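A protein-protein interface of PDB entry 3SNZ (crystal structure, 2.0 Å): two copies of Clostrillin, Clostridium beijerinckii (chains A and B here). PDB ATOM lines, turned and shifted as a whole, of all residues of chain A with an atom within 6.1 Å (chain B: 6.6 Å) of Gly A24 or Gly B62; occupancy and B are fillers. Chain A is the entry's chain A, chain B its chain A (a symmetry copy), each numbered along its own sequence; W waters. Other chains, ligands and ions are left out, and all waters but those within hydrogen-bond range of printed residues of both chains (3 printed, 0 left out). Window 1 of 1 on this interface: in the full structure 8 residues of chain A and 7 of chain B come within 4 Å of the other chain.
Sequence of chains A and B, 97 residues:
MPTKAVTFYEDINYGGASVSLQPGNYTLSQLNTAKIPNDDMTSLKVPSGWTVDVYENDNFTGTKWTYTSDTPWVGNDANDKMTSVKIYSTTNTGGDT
The side-chain amide nitrogen (NE2) of Gln A30 sits close to the side-chain amide nitrogen (ND2) of Asn B57 (3.0 Å).
The side-chain amide nitrogen (ND2) of Asn A25 is in hydrogen-bond range of the backbone carbonyl oxygen (O) of Phe B60 (3.2 Å).
The side-chain hydroxyl (OG1) of Thr B63 sits at hydrogen-bond distance from the side-chain hydroxyl (OH) of Tyr A26 (3.0 Å).
The side-chain amide nitrogen (NE2) of Gln A30 is in hydrogen-bond range of the side-chain hydroxyl (OG1) of Thr B61, 2.9 Å away.
The backbone NH (N) of Lys B64 is in hydrogen-bond range of the backbone carbonyl oxygen (O) of Pro A23 (2.9 Å).
N of Gly B62 is in hydrogen-bond range of O of Asn A25.
The side-chain amide oxygen (OE1) of Gln A30 is in hydrogen-bond range of the backbone NH (N) of Gly B62.
Water W3 lies within hydrogen-bond range of the side-chain hydroxyl (OG1) of Thr B61 (2.5 Å) and the side-chain amide nitrogen (NE2) of Gln A30 (3.3 Å).
Water W1 lies within hydrogen-bond range of O of Phe B60 (2.6 Å) and ND2 of Asn A25 (3.5 Å).
Water W2 lies within hydrogen-bond range of NZ of Lys B64 (2.8 Å), O of Ile A87 (2.9 Å) and OD1 of Asn A25 (2.9 Å).
The backbone carbonyl oxygen (O) of Gly A24 sits at hydrogen-bond distance from the backbone NH (N) of Ile A87, 2.9 Å away.
The backbone carbonyl oxygen (O) of Gln A22 is in hydrogen-bond range of the side-chain hydroxyl (OH) of Tyr A26 (2.6 Å).
The backbone NH (N) of Glu B56 lies within hydrogen-bond range of the backbone carbonyl oxygen (O) of Thr B63 (2.8 Å).
O of Asn A25 sits close to OE1 of Gln A30, 3.3 Å away.
The backbone carbonyl oxygen (O) of Pro A23 lies within hydrogen-bond range of the side-chain hydroxyl (OH) of Tyr A26 (3.4 Å).
N of Thr A27 lies within hydrogen-bond range of OE1 of Gln A30 (3.0 Å).
Of the 11 printed residues of chain A, 8 touch a printed residue of chain B.
Printed residues of chain B that touch a printed residue of chain A: Tyr B55, Asn B57, Phe B60, Thr B61, Gly B62, Thr B63 and Lys B64.
Hydrophobic or aromatic side chains of chain B that line the printed part of chain A: Tyr B55.
Among the printed residues, no Asp or Glu carboxylate lies within 4 Å of a Lys or Arg side-chain nitrogen of the other chain.
No position is printed for both chains.
Of the 16 pairs that touch across the chains among the printed residues, none has its exchanged pair printed and touching as well.
Among the printed residues, merely in contact across the chains: Asn A25 with Thr B61 (3.2 Å), Gly A24 with Gly B62 (3.2 Å), Pro A23 with Thr B63 (3.4 Å), Asn A25 with Tyr B55 (3.5 Å), Tyr A88 with Lys B64 (3.6 Å), Gly A24 with Lys B64 (3.7 Å), Tyr A26 with Gly B62 (3.8 Å), Gln A22 with Thr B63 (3.98 Å) and Thr A27 with Thr B61 (3.99 Å).
Printed residues of chain B within 4 Å of Gln A22: Thr B63 (3.98 Å).
Printed residues of chain B within 4 Å of Pro A23: Thr B63 and Lys B64.
Of the printed residues of chain B, Gln A30 touches Asn B57 (3.0 Å), Thr B61 (2.9 Å) and Gly B62 (3.3 Å).
Val A85 touches none of the printed residues of chain B.
Lys A86 touches none of the printed residues of chain B.
Of the printed residues of chain A, Phe B60 touches Asn A25.
Gly B62 touches just these residues of chain A: Gly A24 (3.2 Å), Asn A25 (2.8 Å), Tyr A26 (3.8 Å) and Gln A30 (3.3 Å).
Of the printed residues of chain A, Lys B64 touches Pro A23 (2.9 Å), Gly A24 (3.7 Å) and Tyr A88 (3.6 Å).
The nearest residue of chain A that does not touch Gly B62 is Pro A23 (4.6 Å).
The nearest printed residue of chain A that does not touch Asn B57 is Tyr A26 (6.1 Å).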
ATOM      1  N   GLN A  22       4.895   5.254 -19.998  1.00  0.00           N
ATOM      2  CA  GLN A  22       4.129   5.061 -18.786  1.00  0.00           C
ATOM      3  C   GLN A  22       2.632   5.127 -19.129  1.00  0.00           C
ATOM      4  O   GLN A  22       2.280   5.502 -20.243  1.00  0.00           O
ATOM      5  CB  GLN A  22       4.508   6.151 -17.775  1.00  0.00           C
ATOM      6  CG  GLN A  22       5.888   5.952 -17.169  1.00  0.00           C
ATOM      7  CD  GLN A  22       6.000   4.618 -16.443  1.00  0.00           C
ATOM      8  OE1 GLN A  22       5.345   4.405 -15.416  1.00  0.00           O
ATOM      9  NE2 GLN A  22       6.825   3.710 -16.973  1.00  0.00           N
ATOM     10  N   PRO A  23       1.750   4.757 -18.181  1.00  0.00           N
ATOM     11  CA  PRO A  23       0.327   4.883 -18.492  1.00  0.00           C
ATOM     12  C   PRO A  23      -0.034   6.297 -18.934  1.00  0.00           C
ATOM     13  O   PRO A  23       0.572   7.268 -18.480  1.00  0.00           O
ATOM     14  CB  PRO A  23      -0.360   4.561 -17.164  1.00  0.00           C
ATOM     15  CG  PRO A  23       0.617   3.747 -16.410  1.00  0.00           C
ATOM     16  CD  PRO A  23       1.976   4.223 -16.823  1.00  0.00           C
ATOM     17  N   GLY A  24      -1.025   6.399 -19.808  1.00  0.00           N
ATOM     18  CA  GLY A  24      -1.477   7.678 -20.336  1.00  0.00           C
ATOM     19  C   GLY A  24      -2.169   7.499 -21.674  1.00  0.00           C
ATOM     20  O   GLY A  24      -2.220   6.395 -22.212  1.00  0.00           O
ATOM     21  N   ASN A  25      -2.693   8.598 -22.205  1.00  0.00           N
ATOM     22  CA  ASN A  25      -3.432   8.598 -23.467  1.00  0.00           C
ATOM     23  C   ASN A  25      -2.637   9.401 -24.487  1.00  0.00           C
ATOM     24  O   ASN A  25      -2.586  10.630 -24.405  1.00  0.00           O
ATOM     25  CB  ASN A  25      -4.834   9.200 -23.257  1.00  0.00           C
ATOM     26  CG  ASN A  25      -5.623   8.489 -22.164  1.00  0.00           C
ATOM     27  OD1 ASN A  25      -5.462   7.289 -21.936  1.00  0.00           O
ATOM     28  ND2 ASN A  25      -6.480   9.234 -21.480  1.00  0.00           N
ATOM     29  N   TYR A  26      -2.005   8.702 -25.435  1.00  0.00           N
ATOM     30  CA  TYR A  26      -1.036   9.315 -26.357  1.00  0.00           C
ATOM     31  C   TYR A  26      -1.548   9.468 -27.781  1.00  0.00           C
ATOM     32  O   TYR A  26      -1.809   8.476 -28.473  1.00  0.00           O
ATOM     33  CB  TYR A  26       0.299   8.537 -26.366  1.00  0.00           C
ATOM     34  CG  TYR A  26       0.901   8.375 -24.981  1.00  0.00           C
ATOM     35  CD1 TYR A  26       1.755   9.344 -24.450  1.00  0.00           C
ATOM     36  CD2 TYR A  26       0.594   7.259 -24.193  1.00  0.00           C
ATOM     37  CE1 TYR A  26       2.310   9.201 -23.160  1.00  0.00           C
ATOM     38  CE2 TYR A  26       1.131   7.110 -22.903  1.00  0.00           C
ATOM     39  CZ  TYR A  26       1.992   8.077 -22.404  1.00  0.00           C
ATOM     40  OH  TYR A  26       2.513   7.921 -21.139  1.00  0.00           O
ATOM     41  N   THR A  27      -1.664  10.721 -28.209  1.00  0.00           N
ATOM     42  CA  THR A  27      -2.042  11.052 -29.580  1.00  0.00           C
ATOM     43  C   THR A  27      -0.854  10.817 -30.506  1.00  0.00           C
ATOM     44  O   THR A  27       0.277  10.614 -30.040  1.00  0.00           O
ATOM     45  CB  THR A  27      -2.447  12.532 -29.703  1.00  0.00           C
ATOM     46  OG1 THR A  27      -1.314  13.349 -29.373  1.00  0.00           O
ATOM     47  CG2 THR A  27      -3.601  12.851 -28.768  1.00  0.00           C
ATOM     48  N   GLN A  30       1.987  13.189 -29.833  1.00  0.00           N
ATOM     49  CA  GLN A  30       2.732  12.797 -28.649  1.00  0.00           C
ATOM     50  C   GLN A  30       3.620  11.572 -28.878  1.00  0.00           C
ATOM     51  O   GLN A  30       4.750  11.515 -28.367  1.00  0.00           O
ATOM     52  CB  GLN A  30       1.768  12.582 -27.489  1.00  0.00           C
ATOM     53  CG  GLN A  30       1.217  13.892 -26.955  1.00  0.00           C
ATOM     54  CD  GLN A  30      -0.097  13.726 -26.240  1.00  0.00           C
ATOM     55  OE1 GLN A  30      -0.646  12.628 -26.161  1.00  0.00           O
ATOM     56  NE2 GLN A  30      -0.614  14.823 -25.710  1.00  0.00           N
ATOM     57  N   VAL A  85      -2.624   5.605 -28.901  1.00  0.00           N
ATOM     58  CA  VAL A  85      -2.580   4.508 -27.940  1.00  0.00           C
ATOM     59  C   VAL A  85      -2.977   4.958 -26.531  1.00  0.00           C
ATOM     60  O   VAL A  85      -2.614   6.057 -26.084  1.00  0.00           O
ATOM     61  CB  VAL A  85      -1.173   3.797 -27.949  1.00  0.00           C
ATOM     62  CG1 VAL A  85      -0.066   4.737 -27.475  1.00  0.00           C
ATOM     63  CG2 VAL A  85      -1.197   2.507 -27.128  1.00  0.00           C
ATOM     64  N   LYS A  86      -3.754   4.119 -25.853  1.00  0.00           N
ATOM     65  CA  LYS A  86      -4.063   4.340 -24.446  1.00  0.00           C
ATOM     66  C   LYS A  86      -3.433   3.217 -23.640  1.00  0.00           C
ATOM     67  O   LYS A  86      -3.509   2.052 -24.022  1.00  0.00           O
ATOM     68  CB  LYS A  86      -5.570   4.408 -24.207  1.00  0.00           C
ATOM     69  CG  LYS A  86      -6.224   5.648 -24.766  1.00  0.00           C
ATOM     70  CD  LYS A  86      -7.655   5.750 -24.272  1.00  0.00           C
ATOM     71  CE  LYS A  86      -8.300   7.042 -24.706  1.00  0.00           C
ATOM     72  NZ  LYS A  86      -9.686   7.181 -24.154  1.00  0.00           N
ATOM     73  N   ILE A  87      -2.788   3.584 -22.536  1.00  0.00           N
ATOM     74  CA  ILE A  87      -2.099   2.622 -21.677  1.00  0.00           C
ATOM     75  C   ILE A  87      -2.615   2.789 -20.255  1.00  0.00           C
ATOM     76  O   ILE A  87      -2.575   3.892 -19.717  1.00  0.00           O
ATOM     77  CB  ILE A  87      -0.563   2.840 -21.690  1.00  0.00           C
ATOM     78  CG1 ILE A  87      -0.007   2.737 -23.121  1.00  0.00           C
ATOM     79  CG2 ILE A  87       0.116   1.849 -20.753  1.00  0.00           C
ATOM     80  CD1 ILE A  87       1.410   3.289 -23.284  1.00  0.00           C
ATOM     81  N   TYR A  88      -3.097   1.699 -19.658  1.00  0.00           N
ATOM     82  CA  TYR A  88      -3.602   1.732 -18.283  1.00  0.00           C
ATOM     83  C   TYR A  88      -2.775   0.812 -17.398  1.00  0.00           C
ATOM     84  O   TYR A  88      -2.447  -0.303 -17.806  1.00  0.00           O
ATOM     85  CB  TYR A  88      -5.067   1.284 -18.218  1.00  0.00           C
ATOM     86  CG  TYR A  88      -6.001   1.980 -19.176  1.00  0.00           C
ATOM     87  CD1 TYR A  88      -6.681   3.133 -18.797  1.00  0.00           C
ATOM     88  CD2 TYR A  88      -6.226   1.469 -20.457  1.00  0.00           C
ATOM     89  CE1 TYR A  88      -7.555   3.781 -19.672  1.00  0.00           C
ATOM     90  CE2 TYR A  88      -7.088   2.104 -21.340  1.00  0.00           C
ATOM     91  CZ  TYR A  88      -7.751   3.260 -20.942  1.00  0.00           C
ATOM     92  OH  TYR A  88      -8.619   3.897 -21.806  1.00  0.00           O
ATOM     93  N   VAL B  54      -4.214  12.850 -13.083  1.00  0.00           N
ATOM     94  CA  VAL B  54      -3.416  13.979 -13.503  1.00  0.00           C
ATOM     95  C   VAL B  54      -2.788  13.669 -14.852  1.00  0.00           C
ATOM     96  O   VAL B  54      -2.140  12.627 -15.009  1.00  0.00           O
ATOM     97  CB  VAL B  54      -2.302  14.239 -12.458  1.00  0.00           C
ATOM     98  CG1 VAL B  54      -1.337  15.309 -12.931  1.00  0.00           C
ATOM     99  CG2 VAL B  54      -2.934  14.616 -11.093  1.00  0.00           C
ATOM    100  N   TYR B  55      -2.968  14.574 -15.812  1.00  0.00           N
ATOM    101  CA  TYR B  55      -2.437  14.380 -17.164  1.00  0.00           C
ATOM    102  C   TYR B  55      -1.362  15.390 -17.493  1.00  0.00           C
ATOM    103  O   TYR B  55      -1.490  16.576 -17.163  1.00  0.00           O
ATOM    104  CB  TYR B  55      -3.542  14.483 -18.214  1.00  0.00           C
ATOM    105  CG  TYR B  55      -4.533  13.360 -18.152  1.00  0.00           C
ATOM    106  CD1 TYR B  55      -4.328  12.183 -18.879  1.00  0.00           C
ATOM    107  CD2 TYR B  55      -5.691  13.468 -17.368  1.00  0.00           C
ATOM    108  CE1 TYR B  55      -5.244  11.144 -18.831  1.00  0.00           C
ATOM    109  CE2 TYR B  55      -6.609  12.426 -17.308  1.00  0.00           C
ATOM    110  CZ  TYR B  55      -6.377  11.273 -18.042  1.00  0.00           C
ATOM    111  OH  TYR B  55      -7.292  10.246 -17.997  1.00  0.00           O
ATOM    112  N   GLU B  56      -0.315  14.906 -18.169  1.00  0.00           N
ATOM    113  CA  GLU B  56       0.847  15.718 -18.514  1.00  0.00           C
ATOM    114  C   GLU B  56       0.509  16.750 -19.583  1.00  0.00           C
ATOM    115  O   GLU B  56       1.113  17.821 -19.625  1.00  0.00           O
ATOM    116  CB  GLU B  56       2.019  14.831 -18.981  1.00  0.00           C
ATOM    117  CG  GLU B  56       3.247  15.621 -19.451  1.00  0.00           C
ATOM    118  CD  GLU B  56       4.459  14.740 -19.775  1.00  0.00           C
ATOM    119  OE1 GLU B  56       4.305  13.714 -20.475  1.00  0.00           O
ATOM    120  OE2 GLU B  56       5.568  15.100 -19.334  1.00  0.00           O
ATOM    121  N   ASN B  57      -0.448  16.434 -20.447  1.00  0.00           N
ATOM    122  CA  ASN B  57      -0.798  17.332 -21.532  1.00  0.00           C
ATOM    123  C   ASN B  57      -2.280  17.684 -21.471  1.00  0.00           C
ATOM    124  O   ASN B  57      -3.044  17.118 -20.670  1.00  0.00           O
ATOM    125  CB  ASN B  57      -0.426  16.715 -22.898  1.00  0.00           C
ATOM    126  CG  ASN B  57       1.085  16.548 -23.084  1.00  0.00           C
ATOM    127  OD1 ASN B  57       1.867  17.446 -22.774  1.00  0.00           O
ATOM    128  ND2 ASN B  57       1.491  15.400 -23.591  1.00  0.00           N
ATOM    129  N   ASP B  58      -2.685  18.611 -22.331  1.00  0.00           N
ATOM    130  CA  ASP B  58      -4.039  19.136 -22.282  1.00  0.00           C
ATOM    131  C   ASP B  58      -5.042  18.132 -22.829  1.00  0.00           C
ATOM    132  O   ASP B  58      -4.687  17.199 -23.573  1.00  0.00           O
ATOM    133  CB  ASP B  58      -4.144  20.466 -23.042  1.00  0.00           C
ATOM    134  CG  ASP B  58      -5.355  21.304 -22.612  1.00  0.00           C
ATOM    135  OD1 ASP B  58      -6.068  20.928 -21.647  1.00  0.00           O
ATOM    136  OD2 ASP B  58      -5.587  22.346 -23.252  1.00  0.00           O
ATOM    137  N   PHE B  60      -6.666  15.787 -21.362  1.00  0.00           N
ATOM    138  CA  PHE B  60      -6.583  14.451 -20.785  1.00  0.00           C
ATOM    139  C   PHE B  60      -5.750  13.524 -21.689  1.00  0.00           C
ATOM    140  O   PHE B  60      -6.161  12.411 -22.028  1.00  0.00           O
ATOM    141  CB  PHE B  60      -8.004  13.943 -20.505  1.00  0.00           C
ATOM    142  CG  PHE B  60      -8.935  15.053 -20.080  1.00  0.00           C
ATOM    143  CD1 PHE B  60      -8.734  15.712 -18.865  1.00  0.00           C
ATOM    144  CD2 PHE B  60      -9.951  15.497 -20.927  1.00  0.00           C
ATOM    145  CE1 PHE B  60      -9.560  16.780 -18.476  1.00  0.00           C
ATOM    146  CE2 PHE B  60     -10.779  16.566 -20.551  1.00  0.00           C
ATOM    147  CZ  PHE B  60     -10.576  17.208 -19.321  1.00  0.00           C
ATOM    148  N   THR B  61      -4.579  14.022 -22.086  1.00  0.00           N
ATOM    149  CA  THR B  61      -3.654  13.258 -22.927  1.00  0.00           C
ATOM    150  C   THR B  61      -2.247  13.352 -22.354  1.00  0.00           C
ATOM    151  O   THR B  61      -2.013  14.053 -21.363  1.00  0.00           O
ATOM    152  CB  THR B  61      -3.652  13.708 -24.418  1.00  0.00           C
ATOM    153  OG1 THR B  61      -3.255  15.081 -24.526  1.00  0.00           O
ATOM    154  CG2 THR B  61      -5.005  13.488 -25.093  1.00  0.00           C
ATOM    155  N   GLY B  62      -1.307  12.640 -22.973  1.00  0.00           N
ATOM    156  CA  GLY B  62       0.027  12.506 -22.403  1.00  0.00           C
ATOM    157  C   GLY B  62       0.016  11.497 -21.275  1.00  0.00           C
ATOM    158  O   GLY B  62      -0.967  10.762 -21.100  1.00  0.00           O
ATOM    159  N   THR B  63       1.102  11.467 -20.506  1.00  0.00           N
ATOM    160  CA  THR B  63       1.227  10.597 -19.341  1.00  0.00           C
ATOM    161  C   THR B  63       0.203  10.935 -18.263  1.00  0.00           C
ATOM    162  O   THR B  63      -0.094  12.110 -18.011  1.00  0.00           O
ATOM    163  CB  THR B  63       2.651  10.672 -18.724  1.00  0.00           C
ATOM    164  OG1 THR B  63       3.611  10.311 -19.718  1.00  0.00           O
ATOM    165  CG2 THR B  63       2.786   9.726 -17.539  1.00  0.00           C
ATOM    166  N   LYS B  64      -0.306   9.890 -17.618  1.00  0.00           N
ATOM    167  CA  LYS B  64      -1.352  10.021 -16.624  1.00  0.00           C
ATOM    168  C   LYS B  64      -0.866   9.450 -15.294  1.00  0.00           C
ATOM    169  O   LYS B  64      -0.410   8.305 -15.242  1.00  0.00           O
ATOM    170  CB  LYS B  64      -2.594   9.279 -17.114  1.00  0.00           C
ATOM    171  CG  LYS B  64      -3.774   9.302 -16.158  1.00  0.00           C
ATOM    172  CD  LYS B  64      -4.851   8.324 -16.618  1.00  0.00           C
ATOM    173  CE  LYS B  64      -4.537   6.897 -16.202  1.00  0.00           C
ATOM    174  NZ  LYS B  64      -5.450   5.920 -16.873  1.00  0.00           N
HETATM  175  O   HOH W   1      -7.958  11.479 -23.667  1.00  0.00           O
HETATM  176  O   HOH W   2      -4.519   6.007 -19.523  1.00  0.00           O
HETATM  177  O   HOH W   3      -3.443  16.281 -26.749  1.00  0.00           O
